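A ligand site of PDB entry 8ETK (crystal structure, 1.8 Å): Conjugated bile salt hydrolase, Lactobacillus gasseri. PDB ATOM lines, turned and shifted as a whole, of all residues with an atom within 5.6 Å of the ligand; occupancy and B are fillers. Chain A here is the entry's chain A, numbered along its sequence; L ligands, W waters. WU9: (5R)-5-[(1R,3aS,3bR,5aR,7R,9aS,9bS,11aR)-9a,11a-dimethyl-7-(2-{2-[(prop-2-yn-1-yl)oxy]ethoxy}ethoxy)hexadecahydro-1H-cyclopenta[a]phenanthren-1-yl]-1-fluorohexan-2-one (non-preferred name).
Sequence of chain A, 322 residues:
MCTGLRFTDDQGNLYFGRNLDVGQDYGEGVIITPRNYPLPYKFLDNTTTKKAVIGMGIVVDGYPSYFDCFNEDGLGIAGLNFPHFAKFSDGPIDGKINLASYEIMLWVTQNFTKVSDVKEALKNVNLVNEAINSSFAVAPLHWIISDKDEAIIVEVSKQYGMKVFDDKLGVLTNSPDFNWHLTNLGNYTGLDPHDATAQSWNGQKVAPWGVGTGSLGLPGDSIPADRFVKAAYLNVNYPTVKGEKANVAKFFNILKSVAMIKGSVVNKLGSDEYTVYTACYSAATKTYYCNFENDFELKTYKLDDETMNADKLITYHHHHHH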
ATOM      1  N   CYS A   2      23.752   3.220  -4.918  1.00  0.00           N
ATOM      2  CA  CYS A   2      25.169   3.605  -4.980  1.00  0.00           C
ATOM      3  C   CYS A   2      25.741   3.754  -3.591  1.00  0.00           C
ATOM      4  O   CYS A   2      25.055   4.207  -2.663  1.00  0.00           O
ATOM      5  CB  CYS A   2      25.364   4.935  -5.736  1.00  0.00           C
ATOM      6  SG  CYS A   2      25.081   4.863  -7.499  1.00  0.00           S
ATOM      7  N   ARG A  18      33.375   4.317  -5.847  1.00  0.00           N
ATOM      8  CA  ARG A  18      31.939   4.125  -5.669  1.00  0.00           C
ATOM      9  C   ARG A  18      31.468   2.897  -6.430  1.00  0.00           C
ATOM     10  O   ARG A  18      32.102   2.447  -7.397  1.00  0.00           O
ATOM     11  CB  ARG A  18      31.144   5.373  -6.137  1.00  0.00           C
ATOM     12  CG  ARG A  18      31.350   5.766  -7.596  1.00  0.00           C
ATOM     13  CD  ARG A  18      30.270   5.171  -8.542  1.00  0.00           C
ATOM     14  NE  ARG A  18      28.935   5.724  -8.252  1.00  0.00           N
ATOM     15  CZ  ARG A  18      28.528   6.948  -8.550  1.00  0.00           C
ATOM     16  NH1 ARG A  18      29.323   7.809  -9.186  1.00  0.00           N
ATOM     17  NH2 ARG A  18      27.296   7.331  -8.212  1.00  0.00           N
ATOM     18  N   ASN A  19      30.336   2.346  -5.966  1.00  0.00           N
ATOM     19  CA  ASN A  19      29.475   1.469  -6.775  1.00  0.00           C
ATOM     20  C   ASN A  19      28.471   2.334  -7.533  1.00  0.00           C
ATOM     21  O   ASN A  19      27.918   3.296  -6.978  1.00  0.00           O
ATOM     22  CB  ASN A  19      28.658   0.505  -5.908  1.00  0.00           C
ATOM     23  CG  ASN A  19      29.489  -0.611  -5.286  1.00  0.00           C
ATOM     24  OD1 ASN A  19      30.553  -0.970  -5.797  1.00  0.00           O
ATOM     25  ND2 ASN A  19      28.989  -1.174  -4.193  1.00  0.00           N
ATOM     26  N   LEU A  20      28.174   1.969  -8.763  1.00  0.00           N
ATOM     27  CA  LEU A  20      27.077   2.570  -9.507  1.00  0.00           C
ATOM     28  C   LEU A  20      25.948   1.555  -9.559  1.00  0.00           C
ATOM     29  O   LEU A  20      26.040   0.561 -10.290  1.00  0.00           O
ATOM     30  CB  LEU A  20      27.497   2.987 -10.918  1.00  0.00           C
ATOM     31  CG  LEU A  20      26.368   3.732 -11.649  1.00  0.00           C
ATOM     32  CD1 LEU A  20      26.347   5.174 -11.183  1.00  0.00           C
ATOM     33  CD2 LEU A  20      26.487   3.688 -13.180  1.00  0.00           C
ATOM     34  N   ASP A  21      24.887   1.796  -8.783  1.00  0.00           N
ATOM     35  CA  ASP A  21      23.743   0.881  -8.690  1.00  0.00           C
ATOM     36  C   ASP A  21      22.578   1.511  -9.440  1.00  0.00           C
ATOM     37  O   ASP A  21      22.015   2.485  -8.955  1.00  0.00           O
ATOM     38  CB  ASP A  21      23.347   0.622  -7.232  1.00  0.00           C
ATOM     39  CG  ASP A  21      24.517   0.148  -6.338  1.00  0.00           C
ATOM     40  OD1 ASP A  21      25.583  -0.236  -6.870  1.00  0.00           O
ATOM     41  OD2 ASP A  21      24.362   0.138  -5.092  1.00  0.00           O
ATOM     42  N   VAL A  22      22.201   0.964 -10.605  1.00  0.00           N
ATOM     43  CA  VAL A  22      21.192   1.610 -11.445  1.00  0.00           C
ATOM     44  C   VAL A  22      20.242   0.592 -12.065  1.00  0.00           C
ATOM     45  O   VAL A  22      20.512  -0.615 -12.116  1.00  0.00           O
ATOM     46  CB  VAL A  22      21.832   2.484 -12.559  1.00  0.00           C
ATOM     47  CG1 VAL A  22      22.480   3.750 -11.976  1.00  0.00           C
ATOM     48  CG2 VAL A  22      22.849   1.695 -13.345  1.00  0.00           C
ATOM     49  N   TYR A  26      23.228   3.943 -19.020  1.00  0.00           N
ATOM     50  CA  TYR A  26      23.443   5.343 -19.397  1.00  0.00           C
ATOM     51  C   TYR A  26      24.476   5.515 -20.499  1.00  0.00           C
ATOM     52  O   TYR A  26      24.713   6.650 -20.924  1.00  0.00           O
ATOM     53  CB  TYR A  26      23.848   6.161 -18.165  1.00  0.00           C
ATOM     54  CG  TYR A  26      22.719   6.285 -17.182  1.00  0.00           C
ATOM     55  CD1 TYR A  26      22.486   5.295 -16.233  1.00  0.00           C
ATOM     56  CD2 TYR A  26      21.843   7.370 -17.224  1.00  0.00           C
ATOM     57  CE1 TYR A  26      21.430   5.396 -15.338  1.00  0.00           C
ATOM     58  CE2 TYR A  26      20.799   7.473 -16.351  1.00  0.00           C
ATOM     59  CZ  TYR A  26      20.598   6.487 -15.402  1.00  0.00           C
ATOM     60  OH  TYR A  26      19.541   6.598 -14.535  1.00  0.00           O
ATOM     61  N   ILE A  58      29.721  10.518 -19.428  1.00  0.00           N
ATOM     62  CA  ILE A  58      29.347  10.643 -20.823  1.00  0.00           C
ATOM     63  C   ILE A  58      29.862  11.985 -21.316  1.00  0.00           C
ATOM     64  O   ILE A  58      30.210  12.864 -20.538  1.00  0.00           O
ATOM     65  CB  ILE A  58      27.820  10.531 -21.069  1.00  0.00           C
ATOM     66  CG1 ILE A  58      27.066  11.638 -20.351  1.00  0.00           C
ATOM     67  CG2 ILE A  58      27.286   9.160 -20.585  1.00  0.00           C
ATOM     68  CD1 ILE A  58      25.635  11.818 -20.857  1.00  0.00           C
ATOM     69  N   SER A  65      30.773  14.894 -18.852  1.00  0.00           N
ATOM     70  CA  SER A  65      29.801  14.933 -17.761  1.00  0.00           C
ATOM     71  C   SER A  65      30.039  13.710 -16.875  1.00  0.00           C
ATOM     72  O   SER A  65      29.615  12.600 -17.199  1.00  0.00           O
ATOM     73  CB  SER A  65      28.373  14.943 -18.309  1.00  0.00           C
ATOM     74  OG  SER A  65      28.192  15.955 -19.278  1.00  0.00           O
ATOM     75  N   TYR A  66      30.703  13.935 -15.741  1.00  0.00           N
ATOM     76  CA  TYR A  66      31.234  12.858 -14.926  1.00  0.00           C
ATOM     77  C   TYR A  66      30.224  12.349 -13.898  1.00  0.00           C
ATOM     78  O   TYR A  66      29.515  13.147 -13.267  1.00  0.00           O
ATOM     79  CB  TYR A  66      32.502  13.328 -14.209  1.00  0.00           C
ATOM     80  CG  TYR A  66      33.754  13.271 -15.068  1.00  0.00           C
ATOM     81  CD1 TYR A  66      34.299  12.041 -15.466  1.00  0.00           C
ATOM     82  CD2 TYR A  66      34.391  14.440 -15.484  1.00  0.00           C
ATOM     83  CE1 TYR A  66      35.458  11.978 -16.246  1.00  0.00           C
ATOM     84  CE2 TYR A  66      35.555  14.390 -16.260  1.00  0.00           C
ATOM     85  CZ  TYR A  66      36.075  13.165 -16.643  1.00  0.00           C
ATOM     86  OH  TYR A  66      37.217  13.136 -17.410  1.00  0.00           O
ATOM     87  N   PHE A  67      30.133  11.021 -13.758  1.00  0.00           N
ATOM     88  CA  PHE A  67      29.465  10.407 -12.619  1.00  0.00           C
ATOM     89  C   PHE A  67      30.344  10.489 -11.371  1.00  0.00           C
ATOM     90  O   PHE A  67      29.851  10.579 -10.248  1.00  0.00           O
ATOM     91  CB  PHE A  67      29.163   8.927 -12.876  1.00  0.00           C
ATOM     92  CG  PHE A  67      28.298   8.630 -14.099  1.00  0.00           C
ATOM     93  CD1 PHE A  67      27.899   9.622 -14.986  1.00  0.00           C
ATOM     94  CD2 PHE A  67      27.898   7.320 -14.339  1.00  0.00           C
ATOM     95  CE1 PHE A  67      27.113   9.294 -16.097  1.00  0.00           C
ATOM     96  CE2 PHE A  67      27.109   6.997 -15.437  1.00  0.00           C
ATOM     97  CZ  PHE A  67      26.727   8.001 -16.331  1.00  0.00           C
ATOM     98  N   GLY A  79      29.116  11.904  -7.621  1.00  0.00           N
ATOM     99  CA  GLY A  79      27.715  12.275  -7.513  1.00  0.00           C
ATOM    100  C   GLY A  79      26.870  11.033  -7.336  1.00  0.00           C
ATOM    101  O   GLY A  79      26.997  10.068  -8.100  1.00  0.00           O
ATOM    102  N   LEU A  80      26.038  11.041  -6.297  1.00  0.00           N
ATOM    103  CA  LEU A  80      25.124   9.955  -6.004  1.00  0.00           C
ATOM    104  C   LEU A  80      23.704  10.513  -5.974  1.00  0.00           C
ATOM    105  O   LEU A  80      23.500  11.686  -5.673  1.00  0.00           O
ATOM    106  CB  LEU A  80      25.455   9.266  -4.668  1.00  0.00           C
ATOM    107  CG  LEU A  80      26.617   8.261  -4.656  1.00  0.00           C
ATOM    108  CD1 LEU A  80      27.949   8.979  -4.888  1.00  0.00           C
ATOM    109  CD2 LEU A  80      26.696   7.456  -3.358  1.00  0.00           C
ATOM    110  N   ASN A  81      22.729   9.658  -6.297  1.00  0.00           N
ATOM    111  CA  ASN A  81      21.338  10.098  -6.259  1.00  0.00           C
ATOM    112  C   ASN A  81      20.853  10.431  -4.853  1.00  0.00           C
ATOM    113  O   ASN A  81      21.199   9.765  -3.873  1.00  0.00           O
ATOM    114  CB  ASN A  81      20.410   9.056  -6.880  1.00  0.00           C
ATOM    115  CG  ASN A  81      19.536   9.644  -7.942  1.00  0.00           C
ATOM    116  OD1 ASN A  81      19.873  10.649  -8.571  1.00  0.00           O
ATOM    117  ND2 ASN A  81      18.410   8.993  -8.190  1.00  0.00           N
ATOM    118  N   TYR A 102      25.273  20.323 -12.458  1.00  0.00           N
ATOM    119  CA  TYR A 102      26.199  19.423 -13.162  1.00  0.00           C
ATOM    120  C   TYR A 102      27.623  19.966 -13.230  1.00  0.00           C
ATOM    121  O   TYR A 102      28.576  19.198 -13.470  1.00  0.00           O
ATOM    122  CB  TYR A 102      25.683  19.102 -14.587  1.00  0.00           C
ATOM    123  CG  TYR A 102      25.892  20.211 -15.597  1.00  0.00           C
ATOM    124  CD1 TYR A 102      24.940  21.202 -15.787  1.00  0.00           C
ATOM    125  CD2 TYR A 102      27.059  20.276 -16.362  1.00  0.00           C
ATOM    126  CE1 TYR A 102      25.123  22.224 -16.700  1.00  0.00           C
ATOM    127  CE2 TYR A 102      27.259  21.310 -17.282  1.00  0.00           C
ATOM    128  CZ  TYR A 102      26.282  22.278 -17.447  1.00  0.00           C
ATOM    129  OH  TYR A 102      26.464  23.300 -18.360  1.00  0.00           O
ATOM    130  N   ALA A 131      20.017  22.229 -16.539  1.00  0.00           N
ATOM    131  CA  ALA A 131      20.698  21.130 -17.217  1.00  0.00           C
ATOM    132  C   ALA A 131      21.694  21.650 -18.261  1.00  0.00           C
ATOM    133  O   ALA A 131      21.708  22.830 -18.623  1.00  0.00           O
ATOM    134  CB  ALA A 131      19.680  20.208 -17.894  1.00  0.00           C
ATOM    135  N   ILE A 132      22.546  20.745 -18.749  1.00  0.00           N
ATOM    136  CA  ILE A 132      23.568  21.160 -19.706  1.00  0.00           C
ATOM    137  C   ILE A 132      22.911  21.678 -20.979  1.00  0.00           C
ATOM    138  O   ILE A 132      23.327  22.689 -21.558  1.00  0.00           O
ATOM    139  CB  ILE A 132      24.559  20.008 -19.974  1.00  0.00           C
ATOM    140  CG1 ILE A 132      25.669  20.496 -20.920  1.00  0.00           C
ATOM    141  CG2 ILE A 132      23.849  18.771 -20.499  1.00  0.00           C
ATOM    142  CD1 ILE A 132      26.977  19.730 -20.775  1.00  0.00           C
ATOM    143  N   PHE A 136      18.286  17.216 -21.631  1.00  0.00           N
ATOM    144  CA  PHE A 136      18.650  16.524 -20.394  1.00  0.00           C
ATOM    145  C   PHE A 136      17.819  17.055 -19.245  1.00  0.00           C
ATOM    146  O   PHE A 136      17.551  18.248 -19.156  1.00  0.00           O
ATOM    147  CB  PHE A 136      20.134  16.719 -20.082  1.00  0.00           C
ATOM    148  CG  PHE A 136      21.028  15.875 -20.935  1.00  0.00           C
ATOM    149  CD1 PHE A 136      21.284  14.559 -20.587  1.00  0.00           C
ATOM    150  CD2 PHE A 136      21.552  16.375 -22.107  1.00  0.00           C
ATOM    151  CE1 PHE A 136      22.070  13.773 -21.390  1.00  0.00           C
ATOM    152  CE2 PHE A 136      22.356  15.579 -22.925  1.00  0.00           C
ATOM    153  CZ  PHE A 136      22.613  14.281 -22.560  1.00  0.00           C
ATOM    154  N   ALA A 137      17.419  16.159 -18.346  1.00  0.00           N
ATOM    155  CA  ALA A 137      16.859  16.570 -17.078  1.00  0.00           C
ATOM    156  C   ALA A 137      17.985  16.848 -16.081  1.00  0.00           C
ATOM    157  O   ALA A 137      19.128  16.435 -16.275  1.00  0.00           O
ATOM    158  CB  ALA A 137      15.915  15.493 -16.523  1.00  0.00           C
ATOM    159  N   VAL A 138      17.637  17.546 -15.008  1.00  0.00           N
ATOM    160  CA  VAL A 138      18.589  17.800 -13.924  1.00  0.00           C
ATOM    161  C   VAL A 138      18.606  16.596 -12.996  1.00  0.00           C
ATOM    162  O   VAL A 138      17.558  16.150 -12.519  1.00  0.00           O
ATOM    163  CB  VAL A 138      18.222  19.094 -13.182  1.00  0.00           C
ATOM    164  CG1 VAL A 138      19.124  19.309 -11.971  1.00  0.00           C
ATOM    165  CG2 VAL A 138      18.302  20.283 -14.133  1.00  0.00           C
ATOM    166  N   ALA A 139      19.783  16.048 -12.729  1.00  0.00           N
ATOM    167  CA  ALA A 139      19.859  14.872 -11.858  1.00  0.00           C
ATOM    168  C   ALA A 139      19.788  15.299 -10.400  1.00  0.00           C
ATOM    169  O   ALA A 139      20.487  16.238  -9.996  1.00  0.00           O
ATOM    170  CB  ALA A 139      21.146  14.096 -12.121  1.00  0.00           C
ATOM    171  N   LEU A 141      21.147  15.084  -7.410  1.00  0.00           N
ATOM    172  CA  LEU A 141      22.329  14.473  -6.803  1.00  0.00           C
ATOM    173  C   LEU A 141      22.650  15.052  -5.431  1.00  0.00           C
ATOM    174  O   LEU A 141      22.281  16.168  -5.097  1.00  0.00           O
ATOM    175  CB  LEU A 141      23.547  14.679  -7.712  1.00  0.00           C
ATOM    176  CG  LEU A 141      23.474  14.069  -9.122  1.00  0.00           C
ATOM    177  CD1 LEU A 141      24.773  14.410  -9.889  1.00  0.00           C
ATOM    178  CD2 LEU A 141      23.283  12.566  -9.073  1.00  0.00           C
ATOM    179  N   ASN A 174      22.397   6.858  -0.425  1.00  0.00           N
ATOM    180  CA  ASN A 174      21.370   7.673  -1.062  1.00  0.00           C
ATOM    181  C   ASN A 174      20.440   8.225   0.005  1.00  0.00           C
ATOM    182  O   ASN A 174      20.879   8.490   1.125  1.00  0.00           O
ATOM    183  CB  ASN A 174      20.618   6.853  -2.113  1.00  0.00           C
ATOM    184  CG  ASN A 174      21.555   6.226  -3.133  1.00  0.00           C
ATOM    185  OD1 ASN A 174      21.789   5.012  -3.120  1.00  0.00           O
ATOM    186  ND2 ASN A 174      22.078   7.042  -4.037  1.00  0.00           N
HETATM  187  C14 WU9 L   1      22.327  10.707 -15.098  1.00  0.00           C
HETATM  188  C11 WU9 L   1      23.665  12.394 -16.551  1.00  0.00           C
HETATM  189  C8  WU9 L   1      22.650  15.221 -16.693  1.00  0.00           C
HETATM  190  C9  WU9 L   1      21.695  14.051 -16.707  1.00  0.00           C
HETATM  191  C10 WU9 L   1      22.375  12.806 -17.289  1.00  0.00           C
HETATM  192  C12 WU9 L   1      24.325  11.308 -17.405  1.00  0.00           C
HETATM  193  C13 WU9 L   1      23.351  11.854 -15.119  1.00  0.00           C
HETATM  194  C15 WU9 L   1      22.078  10.148 -13.687  1.00  0.00           C
HETATM  195  C16 WU9 L   1      23.382   9.676 -13.047  1.00  0.00           C
HETATM  196  C17 WU9 L   1      24.012   8.524 -13.859  1.00  0.00           C
HETATM  197  C18 WU9 L   1      24.306  10.907 -12.987  1.00  0.00           C
HETATM  198  C19 WU9 L   1      25.474  10.444 -12.121  1.00  0.00           C
HETATM  199  C20 WU9 L   1      24.787   9.585 -11.041  1.00  0.00           C
HETATM  200  C21 WU9 L   1      23.341   9.295 -11.540  1.00  0.00           C
HETATM  201  C22 WU9 L   1      22.848   7.892 -11.103  1.00  0.00           C
HETATM  202  C23 WU9 L   1      21.443   7.530 -11.579  1.00  0.00           C
HETATM  203  C24 WU9 L   1      22.915   7.835  -9.567  1.00  0.00           C
HETATM  204  C25 WU9 L   1      22.265   6.579  -8.980  1.00  0.00           C
HETATM  205  C26 WU9 L   1      22.869   6.292  -7.639  1.00  0.00           C
HETATM  206  C27 WU9 L   1      23.327   4.892  -7.517  1.00  0.00           C
HETATM  207  C28 WU9 L   1      24.648  11.496 -14.360  1.00  0.00           C
HETATM  208  C29 WU9 L   1      25.557  12.726 -14.257  1.00  0.00           C
HETATM  209  C30 WU9 L   1      25.872  13.323 -15.625  1.00  0.00           C
HETATM  210  C31 WU9 L   1      24.598  13.638 -16.422  1.00  0.00           C
HETATM  211  C32 WU9 L   1      23.898  14.888 -15.879  1.00  0.00           C
HETATM  212  O3  WU9 L   1      21.969  16.397 -16.232  1.00  0.00           O
HETATM  213  O4  WU9 L   1      23.079   7.117  -6.777  1.00  0.00           O
HETATM  214  O   HOH W   1      22.176  17.550 -13.846  1.00  0.00           O
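N of Cys 2 lies within hydrogen-bond range of OD1 of Asn 174.
The guanidinium group (NH2) of Arg 18 sits at hydrogen-bond distance from the side-chain sulfur (SG) of Cys 2, at 3.4 Å.
The backbone carbonyl oxygen (O) of Gly 79 is in hydrogen-bond range of the guanidinium group (NH2) of Arg 18.
The backbone carbonyl oxygen of Phe 67 lies within hydrogen-bond range of the backbone NH of Gly 79.
The backbone NH (N) of Cys 2 lies within hydrogen-bond range of the side-chain carboxylate (OD2) of Asp 21 (3.1 Å).
The side-chain amide nitrogen (ND2) of Asn 174 sits at hydrogen-bond distance from the backbone carbonyl oxygen (O) of Asn 81, at 2.9 Å.
The backbone NH (N) of Ser 65 sits at hydrogen-bond distance from the backbone carbonyl oxygen (O) of Ile 58.
The guanidinium group (NH1) of Arg 18 lies within hydrogen-bond range of the backbone carbonyl oxygen (O) of Phe 67 (3.0 Å).
Water W1 bridges an oxygen (O3) of the ligand and the backbone NH of Ala 139.
O of Ala 137 sits close to O3 of the ligand.
Asp 21 touches the ligand (O to C27, 3.1 Å).
Val 22 touches the ligand.
Tyr 26 touches the ligand (OH to C23, 3.6 Å).
CD1 of Ile 58 touches C12 of the ligand (3.7 Å).
Phe 67 touches the ligand (CE1 to C12, 3.7 Å).
O of Gly 79 touches C20 of the ligand, 3.7 Å away.
C of Leu 80 touches O4 of the ligand, at 3.5 Å.
CD1 of Phe 136 touches C10 of the ligand, 3.9 Å away.
CD2 of Leu 141 touches C20 of the ligand (3.9 Å).
Hydrophobic or aromatic side chains that line the ligand: Val 22, Tyr 26, Ile 58, Phe 67, Leu 80, Phe 136 and Leu 141.
Within 4 Å of the ligand: Cys 2, Asp 21, Val 22, Tyr 26, Ile 58, Phe 67, Gly 79, Leu 80, Asn 81, Phe 136, Ala 137, Leu 141 and Asn 174.
The nearest printed residue that does not touch the ligand is Ser 65 (4.01 Å).
The side-chain amide nitrogen (ND2) of Asn 174 lies within hydrogen-bond range of an oxygen (O4) of the ligand.
C27 of the ligand is covalently linked to SG of Cys 2, at 1.8 Å.
An oxygen (O4) of the ligand is in hydrogen-bond range of the backbone NH of Asn 81 (2.6 Å).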
